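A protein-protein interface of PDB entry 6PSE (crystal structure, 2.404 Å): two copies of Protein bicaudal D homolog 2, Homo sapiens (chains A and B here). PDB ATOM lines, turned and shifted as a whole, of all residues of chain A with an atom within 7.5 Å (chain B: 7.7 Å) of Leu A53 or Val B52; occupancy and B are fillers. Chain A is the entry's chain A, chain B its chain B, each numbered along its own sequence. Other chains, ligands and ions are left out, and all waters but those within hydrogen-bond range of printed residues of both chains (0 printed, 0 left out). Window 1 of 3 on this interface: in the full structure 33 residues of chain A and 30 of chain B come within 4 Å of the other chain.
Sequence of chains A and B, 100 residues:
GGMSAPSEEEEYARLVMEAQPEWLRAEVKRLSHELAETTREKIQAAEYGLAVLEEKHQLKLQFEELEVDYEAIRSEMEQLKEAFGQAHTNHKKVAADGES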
ATOM      1  N   GLU A  47      28.709  13.183  -5.054  1.00  0.00           N
ATOM      2  CA  GLU A  47      29.346  14.494  -5.120  1.00  0.00           C
ATOM      3  C   GLU A  47      30.073  14.684  -6.450  1.00  0.00           C
ATOM      4  O   GLU A  47      29.925  15.722  -7.108  1.00  0.00           O
ATOM      5  CB  GLU A  47      30.306  14.670  -3.942  1.00  0.00           C
ATOM      6  CG  GLU A  47      29.636  14.653  -2.577  1.00  0.00           C
ATOM      7  CD  GLU A  47      30.635  14.795  -1.424  1.00  0.00           C
ATOM      8  OE1 GLU A  47      31.858  14.889  -1.702  1.00  0.00           O
ATOM      9  OE2 GLU A  47      30.194  14.815  -0.243  1.00  0.00           O
ATOM     10  N   TYR A  48      30.869  13.688  -6.864  1.00  0.00           N
ATOM     11  CA  TYR A  48      31.524  13.754  -8.169  1.00  0.00           C
ATOM     12  C   TYR A  48      30.516  14.086  -9.261  1.00  0.00           C
ATOM     13  O   TYR A  48      30.749  14.973 -10.093  1.00  0.00           O
ATOM     14  CB  TYR A  48      32.218  12.421  -8.467  1.00  0.00           C
ATOM     15  CG  TYR A  48      33.242  12.433  -9.600  1.00  0.00           C
ATOM     16  CD1 TYR A  48      32.850  12.445 -10.937  1.00  0.00           C
ATOM     17  CD2 TYR A  48      34.605  12.379  -9.327  1.00  0.00           C
ATOM     18  CE1 TYR A  48      33.804  12.430 -11.973  1.00  0.00           C
ATOM     19  CE2 TYR A  48      35.557  12.361 -10.350  1.00  0.00           C
ATOM     20  CZ  TYR A  48      35.153  12.384 -11.666  1.00  0.00           C
ATOM     21  OH  TYR A  48      36.106  12.368 -12.660  1.00  0.00           O
ATOM     22  N   GLY A  49      29.369  13.397  -9.245  1.00  0.00           N
ATOM     23  CA  GLY A  49      28.357  13.618 -10.268  1.00  0.00           C
ATOM     24  C   GLY A  49      27.824  15.038 -10.276  1.00  0.00           C
ATOM     25  O   GLY A  49      27.653  15.650 -11.333  1.00  0.00           O
ATOM     26  N   LEU A  50      27.551  15.587  -9.096  1.00  0.00           N
ATOM     27  CA  LEU A  50      27.087  16.963  -9.050  1.00  0.00           C
ATOM     28  C   LEU A  50      28.169  17.923  -9.538  1.00  0.00           C
ATOM     29  O   LEU A  50      27.866  18.919 -10.205  1.00  0.00           O
ATOM     30  CB  LEU A  50      26.611  17.304  -7.634  1.00  0.00           C
ATOM     31  CG  LEU A  50      25.301  16.555  -7.312  1.00  0.00           C
ATOM     32  CD1 LEU A  50      24.857  16.651  -5.833  1.00  0.00           C
ATOM     33  CD2 LEU A  50      24.163  16.975  -8.252  1.00  0.00           C
ATOM     34  N   ALA A  51      29.436  17.631  -9.246  1.00  0.00           N
ATOM     35  CA  ALA A  51      30.505  18.519  -9.698  1.00  0.00           C
ATOM     36  C   ALA A  51      30.618  18.518 -11.219  1.00  0.00           C
ATOM     37  O   ALA A  51      30.673  19.581 -11.848  1.00  0.00           O
ATOM     38  CB  ALA A  51      31.839  18.116  -9.070  1.00  0.00           C
ATOM     39  N   VAL A  52      30.659  17.333 -11.827  1.00  0.00           N
ATOM     40  CA  VAL A  52      30.801  17.263 -13.277  1.00  0.00           C
ATOM     41  C   VAL A  52      29.524  17.726 -13.960  1.00  0.00           C
ATOM     42  O   VAL A  52      29.573  18.292 -15.061  1.00  0.00           O
ATOM     43  CB  VAL A  52      31.190  15.840 -13.727  1.00  0.00           C
ATOM     44  CG1 VAL A  52      32.617  15.501 -13.297  1.00  0.00           C
ATOM     45  CG2 VAL A  52      30.205  14.825 -13.184  1.00  0.00           C
ATOM     46  N   LEU A  53      28.364  17.495 -13.338  1.00  0.00           N
ATOM     47  CA  LEU A  53      27.132  18.062 -13.877  1.00  0.00           C
ATOM     48  C   LEU A  53      27.227  19.576 -13.930  1.00  0.00           C
ATOM     49  O   LEU A  53      26.813  20.201 -14.911  1.00  0.00           O
ATOM     50  CB  LEU A  53      25.934  17.632 -13.038  1.00  0.00           C
ATOM     51  CG  LEU A  53      24.636  17.325 -13.779  1.00  0.00           C
ATOM     52  CD1 LEU A  53      24.898  16.776 -15.159  1.00  0.00           C
ATOM     53  CD2 LEU A  53      23.840  16.317 -12.968  1.00  0.00           C
ATOM     54  N   GLU A  54      27.804  20.181 -12.893  1.00  0.00           N
ATOM     55  CA  GLU A  54      27.915  21.632 -12.867  1.00  0.00           C
ATOM     56  C   GLU A  54      28.933  22.125 -13.886  1.00  0.00           C
ATOM     57  O   GLU A  54      28.667  23.086 -14.623  1.00  0.00           O
ATOM     58  CB  GLU A  54      28.278  22.110 -11.464  1.00  0.00           C
ATOM     59  CG  GLU A  54      28.274  23.622 -11.333  1.00  0.00           C
ATOM     60  CD  GLU A  54      26.945  24.259 -11.745  1.00  0.00           C
ATOM     61  OE1 GLU A  54      25.896  23.570 -11.738  1.00  0.00           O
ATOM     62  OE2 GLU A  54      26.953  25.464 -12.067  1.00  0.00           O
ATOM     63  N   GLU A  55      30.113  21.487 -13.936  1.00  0.00           N
ATOM     64  CA  GLU A  55      31.097  21.855 -14.946  1.00  0.00           C
ATOM     65  C   GLU A  55      30.471  21.796 -16.322  1.00  0.00           C
ATOM     66  O   GLU A  55      30.629  22.722 -17.126  1.00  0.00           O
ATOM     67  CB  GLU A  55      32.314  20.937 -14.890  1.00  0.00           C
ATOM     68  CG  GLU A  55      33.074  20.919 -13.579  1.00  0.00           C
ATOM     69  CD  GLU A  55      34.115  19.809 -13.537  1.00  0.00           C
ATOM     70  OE1 GLU A  55      34.562  19.392 -14.628  1.00  0.00           O
ATOM     71  OE2 GLU A  55      34.483  19.349 -12.427  1.00  0.00           O
ATOM     72  N   LYS A  56      29.711  20.730 -16.593  1.00  0.00           N
ATOM     73  CA  LYS A  56      29.028  20.640 -17.875  1.00  0.00           C
ATOM     74  C   LYS A  56      28.070  21.805 -18.072  1.00  0.00           C
ATOM     75  O   LYS A  56      28.010  22.387 -19.158  1.00  0.00           O
ATOM     76  CB  LYS A  56      28.286  19.320 -17.999  1.00  0.00           C
ATOM     77  CG  LYS A  56      27.636  19.180 -19.340  1.00  0.00           C
ATOM     78  CD  LYS A  56      27.303  17.747 -19.629  1.00  0.00           C
ATOM     79  CE  LYS A  56      26.136  17.653 -20.588  1.00  0.00           C
ATOM     80  NZ  LYS A  56      24.965  16.968 -19.974  1.00  0.00           N
ATOM     81  N   HIS A  57      27.333  22.182 -17.026  1.00  0.00           N
ATOM     82  CA  HIS A  57      26.407  23.305 -17.149  1.00  0.00           C
ATOM     83  C   HIS A  57      27.138  24.594 -17.505  1.00  0.00           C
ATOM     84  O   HIS A  57      26.712  25.338 -18.395  1.00  0.00           O
ATOM     85  CB  HIS A  57      25.617  23.491 -15.854  1.00  0.00           C
ATOM     86  CG  HIS A  57      24.569  24.556 -15.941  1.00  0.00           C
ATOM     87  ND1 HIS A  57      23.514  24.490 -16.829  1.00  0.00           N
ATOM     88  CD2 HIS A  57      24.425  25.725 -15.273  1.00  0.00           C
ATOM     89  CE1 HIS A  57      22.760  25.565 -16.694  1.00  0.00           C
ATOM     90  NE2 HIS A  57      23.291  26.331 -15.756  1.00  0.00           N
ATOM     91  N   GLN A  58      28.231  24.886 -16.803  1.00  0.00           N
ATOM     92  CA  GLN A  58      28.993  26.087 -17.105  1.00  0.00           C
ATOM     93  C   GLN A  58      29.488  26.066 -18.545  1.00  0.00           C
ATOM     94  O   GLN A  58      29.376  27.069 -19.265  1.00  0.00           O
ATOM     95  CB  GLN A  58      30.168  26.217 -16.131  1.00  0.00           C
ATOM     96  CG  GLN A  58      29.779  26.553 -14.699  1.00  0.00           C
ATOM     97  CD  GLN A  58      28.544  27.443 -14.622  1.00  0.00           C
ATOM     98  OE1 GLN A  58      28.524  28.535 -15.184  1.00  0.00           O
ATOM     99  NE2 GLN A  58      27.507  26.974 -13.927  1.00  0.00           N
ATOM    100  N   LEU A  59      30.023  24.920 -18.983  1.00  0.00           N
ATOM    101  CA  LEU A  59      30.526  24.790 -20.345  1.00  0.00           C
ATOM    102  C   LEU A  59      29.421  25.040 -21.361  1.00  0.00           C
ATOM    103  O   LEU A  59      29.652  25.675 -22.393  1.00  0.00           O
ATOM    104  CB  LEU A  59      31.141  23.402 -20.546  1.00  0.00           C
ATOM    105  CG  LEU A  59      31.680  23.111 -21.950  1.00  0.00           C
ATOM    106  CD1 LEU A  59      32.823  24.051 -22.308  1.00  0.00           C
ATOM    107  CD2 LEU A  59      32.104  21.659 -22.106  1.00  0.00           C
ATOM    108  N   ALA B  46      28.214   5.934 -10.063  1.00  0.00           N
ATOM    109  CA  ALA B  46      29.465   5.997 -10.821  1.00  0.00           C
ATOM    110  C   ALA B  46      29.211   5.943 -12.323  1.00  0.00           C
ATOM    111  O   ALA B  46      29.822   6.694 -13.095  1.00  0.00           O
ATOM    112  CB  ALA B  46      30.398   4.862 -10.409  1.00  0.00           C
ATOM    113  N   GLU B  47      28.304   5.070 -12.758  1.00  0.00           N
ATOM    114  CA  GLU B  47      28.016   4.982 -14.181  1.00  0.00           C
ATOM    115  C   GLU B  47      27.376   6.266 -14.706  1.00  0.00           C
ATOM    116  O   GLU B  47      27.660   6.675 -15.838  1.00  0.00           O
ATOM    117  CB  GLU B  47      27.162   3.741 -14.451  1.00  0.00           C
ATOM    118  CG  GLU B  47      27.880   2.443 -13.966  1.00  0.00           C
ATOM    119  CD  GLU B  47      27.074   1.144 -14.148  1.00  0.00           C
ATOM    120  OE1 GLU B  47      27.695   0.047 -14.148  1.00  0.00           O
ATOM    121  OE2 GLU B  47      25.830   1.212 -14.289  1.00  0.00           O
ATOM    122  N   TYR B  48      26.565   6.953 -13.896  1.00  0.00           N
ATOM    123  CA  TYR B  48      26.066   8.267 -14.310  1.00  0.00           C
ATOM    124  C   TYR B  48      27.182   9.302 -14.384  1.00  0.00           C
ATOM    125  O   TYR B  48      27.184  10.146 -15.285  1.00  0.00           O
ATOM    126  CB  TYR B  48      24.990   8.760 -13.360  1.00  0.00           C
ATOM    127  CG  TYR B  48      23.635   8.210 -13.661  1.00  0.00           C
ATOM    128  CD1 TYR B  48      23.241   7.987 -14.966  1.00  0.00           C
ATOM    129  CD2 TYR B  48      22.745   7.903 -12.636  1.00  0.00           C
ATOM    130  CE1 TYR B  48      21.994   7.474 -15.254  1.00  0.00           C
ATOM    131  CE2 TYR B  48      21.497   7.387 -12.910  1.00  0.00           C
ATOM    132  CZ  TYR B  48      21.124   7.176 -14.225  1.00  0.00           C
ATOM    133  OH  TYR B  48      19.877   6.672 -14.522  1.00  0.00           O
ATOM    134  N   GLY B  49      28.119   9.281 -13.431  1.00  0.00           N
ATOM    135  CA  GLY B  49      29.247  10.199 -13.508  1.00  0.00           C
ATOM    136  C   GLY B  49      30.032  10.045 -14.798  1.00  0.00           C
ATOM    137  O   GLY B  49      30.401  11.030 -15.445  1.00  0.00           O
ATOM    138  N   LEU B  50      30.283   8.797 -15.200  1.00  0.00           N
ATOM    139  CA  LEU B  50      30.989   8.532 -16.448  1.00  0.00           C
ATOM    140  C   LEU B  50      30.226   9.074 -17.655  1.00  0.00           C
ATOM    141  O   LEU B  50      30.828   9.630 -18.580  1.00  0.00           O
ATOM    142  CB  LEU B  50      31.223   7.029 -16.587  1.00  0.00           C
ATOM    143  CG  LEU B  50      32.218   6.646 -17.681  1.00  0.00           C
ATOM    144  CD1 LEU B  50      33.649   6.944 -17.227  1.00  0.00           C
ATOM    145  CD2 LEU B  50      32.048   5.188 -18.087  1.00  0.00           C
ATOM    146  N   ALA B  51      28.897   8.933 -17.657  1.00  0.00           N
ATOM    147  CA  ALA B  51      28.104   9.433 -18.775  1.00  0.00           C
ATOM    148  C   ALA B  51      28.200  10.948 -18.893  1.00  0.00           C
ATOM    149  O   ALA B  51      28.283  11.485 -20.006  1.00  0.00           O
ATOM    150  CB  ALA B  51      26.649   9.004 -18.631  1.00  0.00           C
ATOM    151  N   VAL B  52      28.191  11.666 -17.767  1.00  0.00           N
ATOM    152  CA  VAL B  52      28.343  13.116 -17.856  1.00  0.00           C
ATOM    153  C   VAL B  52      29.719  13.468 -18.405  1.00  0.00           C
ATOM    154  O   VAL B  52      29.848  14.343 -19.270  1.00  0.00           O
ATOM    155  CB  VAL B  52      28.083  13.788 -16.497  1.00  0.00           C
ATOM    156  CG1 VAL B  52      28.484  15.258 -16.555  1.00  0.00           C
ATOM    157  CG2 VAL B  52      26.617  13.645 -16.118  1.00  0.00           C
ATOM    158  N   LEU B  53      30.760  12.769 -17.940  1.00  0.00           N
ATOM    159  CA  LEU B  53      32.096  13.005 -18.484  1.00  0.00           C
ATOM    160  C   LEU B  53      32.120  12.815 -19.995  1.00  0.00           C
ATOM    161  O   LEU B  53      32.701  13.626 -20.725  1.00  0.00           O
ATOM    162  CB  LEU B  53      33.099  12.072 -17.829  1.00  0.00           C
ATOM    163  CG  LEU B  53      33.499  12.403 -16.406  1.00  0.00           C
ATOM    164  CD1 LEU B  53      34.701  11.542 -16.031  1.00  0.00           C
ATOM    165  CD2 LEU B  53      33.826  13.880 -16.316  1.00  0.00           C
ATOM    166  N   GLU B  54      31.495  11.744 -20.480  1.00  0.00           N
ATOM    167  CA  GLU B  54      31.398  11.531 -21.917  1.00  0.00           C
ATOM    168  C   GLU B  54      30.689  12.691 -22.584  1.00  0.00           C
ATOM    169  O   GLU B  54      31.149  13.206 -23.607  1.00  0.00           O
ATOM    170  CB  GLU B  54      30.649  10.236 -22.203  1.00  0.00           C
ATOM    171  CG  GLU B  54      31.504   9.002 -22.190  1.00  0.00           C
ATOM    172  CD  GLU B  54      30.687   7.741 -22.378  1.00  0.00           C
ATOM    173  OE1 GLU B  54      31.068   6.696 -21.797  1.00  0.00           O
ATOM    174  OE2 GLU B  54      29.668   7.804 -23.107  1.00  0.00           O
ATOM    175  N   GLU B  55      29.552  13.105 -22.017  1.00  0.00           N
ATOM    176  CA  GLU B  55      28.796  14.229 -22.567  1.00  0.00           C
ATOM    177  C   GLU B  55      29.626  15.506 -22.566  1.00  0.00           C
ATOM    178  O   GLU B  55      29.679  16.227 -23.570  1.00  0.00           O
ATOM    179  CB  GLU B  55      27.511  14.442 -21.768  1.00  0.00           C
ATOM    180  CG  GLU B  55      26.366  13.524 -22.139  1.00  0.00           C
ATOM    181  CD  GLU B  55      25.303  13.448 -21.048  1.00  0.00           C
ATOM    182  OE1 GLU B  55      25.419  14.190 -20.042  1.00  0.00           O
ATOM    183  OE2 GLU B  55      24.353  12.644 -21.197  1.00  0.00           O
ATOM    184  N   LYS B  56      30.282  15.805 -21.440  1.00  0.00           N
ATOM    185  CA  LYS B  56      31.120  16.997 -21.375  1.00  0.00           C
ATOM    186  C   LYS B  56      32.268  16.935 -22.381  1.00  0.00           C
ATOM    187  O   LYS B  56      32.679  17.968 -22.924  1.00  0.00           O
ATOM    188  CB  LYS B  56      31.651  17.178 -19.958  1.00  0.00           C
ATOM    189  CG  LYS B  56      31.936  18.617 -19.586  1.00  0.00           C
ATOM    190  CD  LYS B  56      32.473  18.749 -18.172  1.00  0.00           C
ATOM    191  CE  LYS B  56      33.592  17.771 -17.944  1.00  0.00           C
ATOM    192  NZ  LYS B  56      34.433  18.208 -16.820  1.00  0.00           N
ATOM    193  N   HIS B  57      32.783  15.738 -22.660  1.00  0.00           N
ATOM    194  CA  HIS B  57      33.845  15.608 -23.652  1.00  0.00           C
ATOM    195  C   HIS B  57      33.350  15.978 -25.044  1.00  0.00           C
ATOM    196  O   HIS B  57      34.026  16.712 -25.777  1.00  0.00           O
ATOM    197  CB  HIS B  57      34.389  14.187 -23.649  1.00  0.00           C
ATOM    198  CG  HIS B  57      35.552  13.981 -24.567  1.00  0.00           C
ATOM    199  ND1 HIS B  57      36.815  14.452 -24.285  1.00  0.00           N
ATOM    200  CD2 HIS B  57      35.644  13.335 -25.757  1.00  0.00           C
ATOM    201  CE1 HIS B  57      37.639  14.100 -25.259  1.00  0.00           C
ATOM    202  NE2 HIS B  57      36.953  13.419 -26.162  1.00  0.00           N
ATOM    203  N   GLN B  58      32.182  15.456 -25.435  1.00  0.00           N
ATOM    204  CA  GLN B  58      31.623  15.815 -26.732  1.00  0.00           C
ATOM    205  C   GLN B  58      31.438  17.321 -26.826  1.00  0.00           C
ATOM    206  O   GLN B  58      31.824  17.952 -27.822  1.00  0.00           O
ATOM    207  CB  GLN B  58      30.296  15.089 -26.964  1.00  0.00           C
ATOM    208  CG  GLN B  58      29.675  15.320 -28.353  1.00  0.00           C
ATOM    209  CD  GLN B  58      28.668  14.243 -28.750  1.00  0.00           C
ATOM    210  OE1 GLN B  58      28.607  13.177 -28.130  1.00  0.00           O
ATOM    211  NE2 GLN B  58      27.859  14.529 -29.772  1.00  0.00           N
ATOM    212  N   LEU B  59      30.894  17.918 -25.764  1.00  0.00           N
ATOM    213  CA  LEU B  59      30.625  19.347 -25.765  1.00  0.00           C
ATOM    214  C   LEU B  59      31.913  20.172 -25.745  1.00  0.00           C
ATOM    215  O   LEU B  59      31.992  21.217 -26.399  1.00  0.00           O
ATOM    216  CB  LEU B  59      29.731  19.683 -24.581  1.00  0.00           C
ATOM    217  CG  LEU B  59      29.408  21.146 -24.297  1.00  0.00           C
ATOM    218  CD1 LEU B  59      28.667  21.778 -25.457  1.00  0.00           C
ATOM    219  CD2 LEU B  59      28.590  21.229 -23.008  1.00  0.00           C
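The side-chain carboxylate (OE1) of Glu A55 is in salt-bridge range of the side-chain amino group (NZ) of Lys B56. The side-chain amino group (NZ) of Lys A56 lies within salt-bridge range of the side-chain carboxylate (OE1) of Glu B55 (2.8 Å).
Among the printed residues, merely in contact across the chains: Tyr A48 with Leu B53 (3.7 Å), Val A52 with Val B52 (3.6 Å), Val A52 with Leu B53 (3.6 Å), Leu A53 with Val B52 (3.7 Å), Lys A56 with Lys B56 (3.7 Å), Leu A59 with Lys B56 (3.8 Å) and Leu A59 with Leu B59 (3.5 Å).
Printed residues of chain A that touch a printed residue of chain B: Tyr A48, Val A52, Leu A53, Glu A55, Lys A56 and Leu A59. Along chain A the printed residues that touch a printed residue of chain B span positions 48 to 59. Of the 14 printed residues of chain B, 5 touch a printed residue of chain A. Among the printed residues, Asp or Glu carboxylates within 4 Å of a Lys or Arg side-chain nitrogen of the other chain: Glu A55 with Lys B56 (2.5 Å) and Lys A56 with Glu B55 (2.8 Å).
Of chain B, only Val B52 comes within 4 Å of Leu A53. Printed residues of chain B within 4 Å of Glu A55: Lys B56 (2.5 Å). Printed residues of chain B within 4 Å of Lys A56: Glu B55 (2.8 Å) and Lys B56 (3.7 Å). Of the printed residues of chain B, Leu A59 touches Lys B56 (3.8 Å) and Leu B59 (3.5 Å). Ala B51 touches none of the printed residues of chain A. Val B52 touches just these residues of chain A: Val A52 and Leu A53. Of the printed residues of chain A, Glu B55 touches Lys A56 (2.8 Å). The nearest residue of chain A that does not touch Val B52 is Lys A56 (4.1 Å). The nearest printed residue of chain B that does not touch Tyr A48 is Gly B49 (5.0 Å).
Tyr A48 touches Leu B53, but with the chains exchanged Leu A53 does not touch Tyr B48 (7.0 Å). Val B52 touches its own counterpart, Val A52. Glu A55 touches Lys B56, and with the chains exchanged Lys A56 touches Glu B55. Leu A59 touches its own counterpart, Leu B59.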
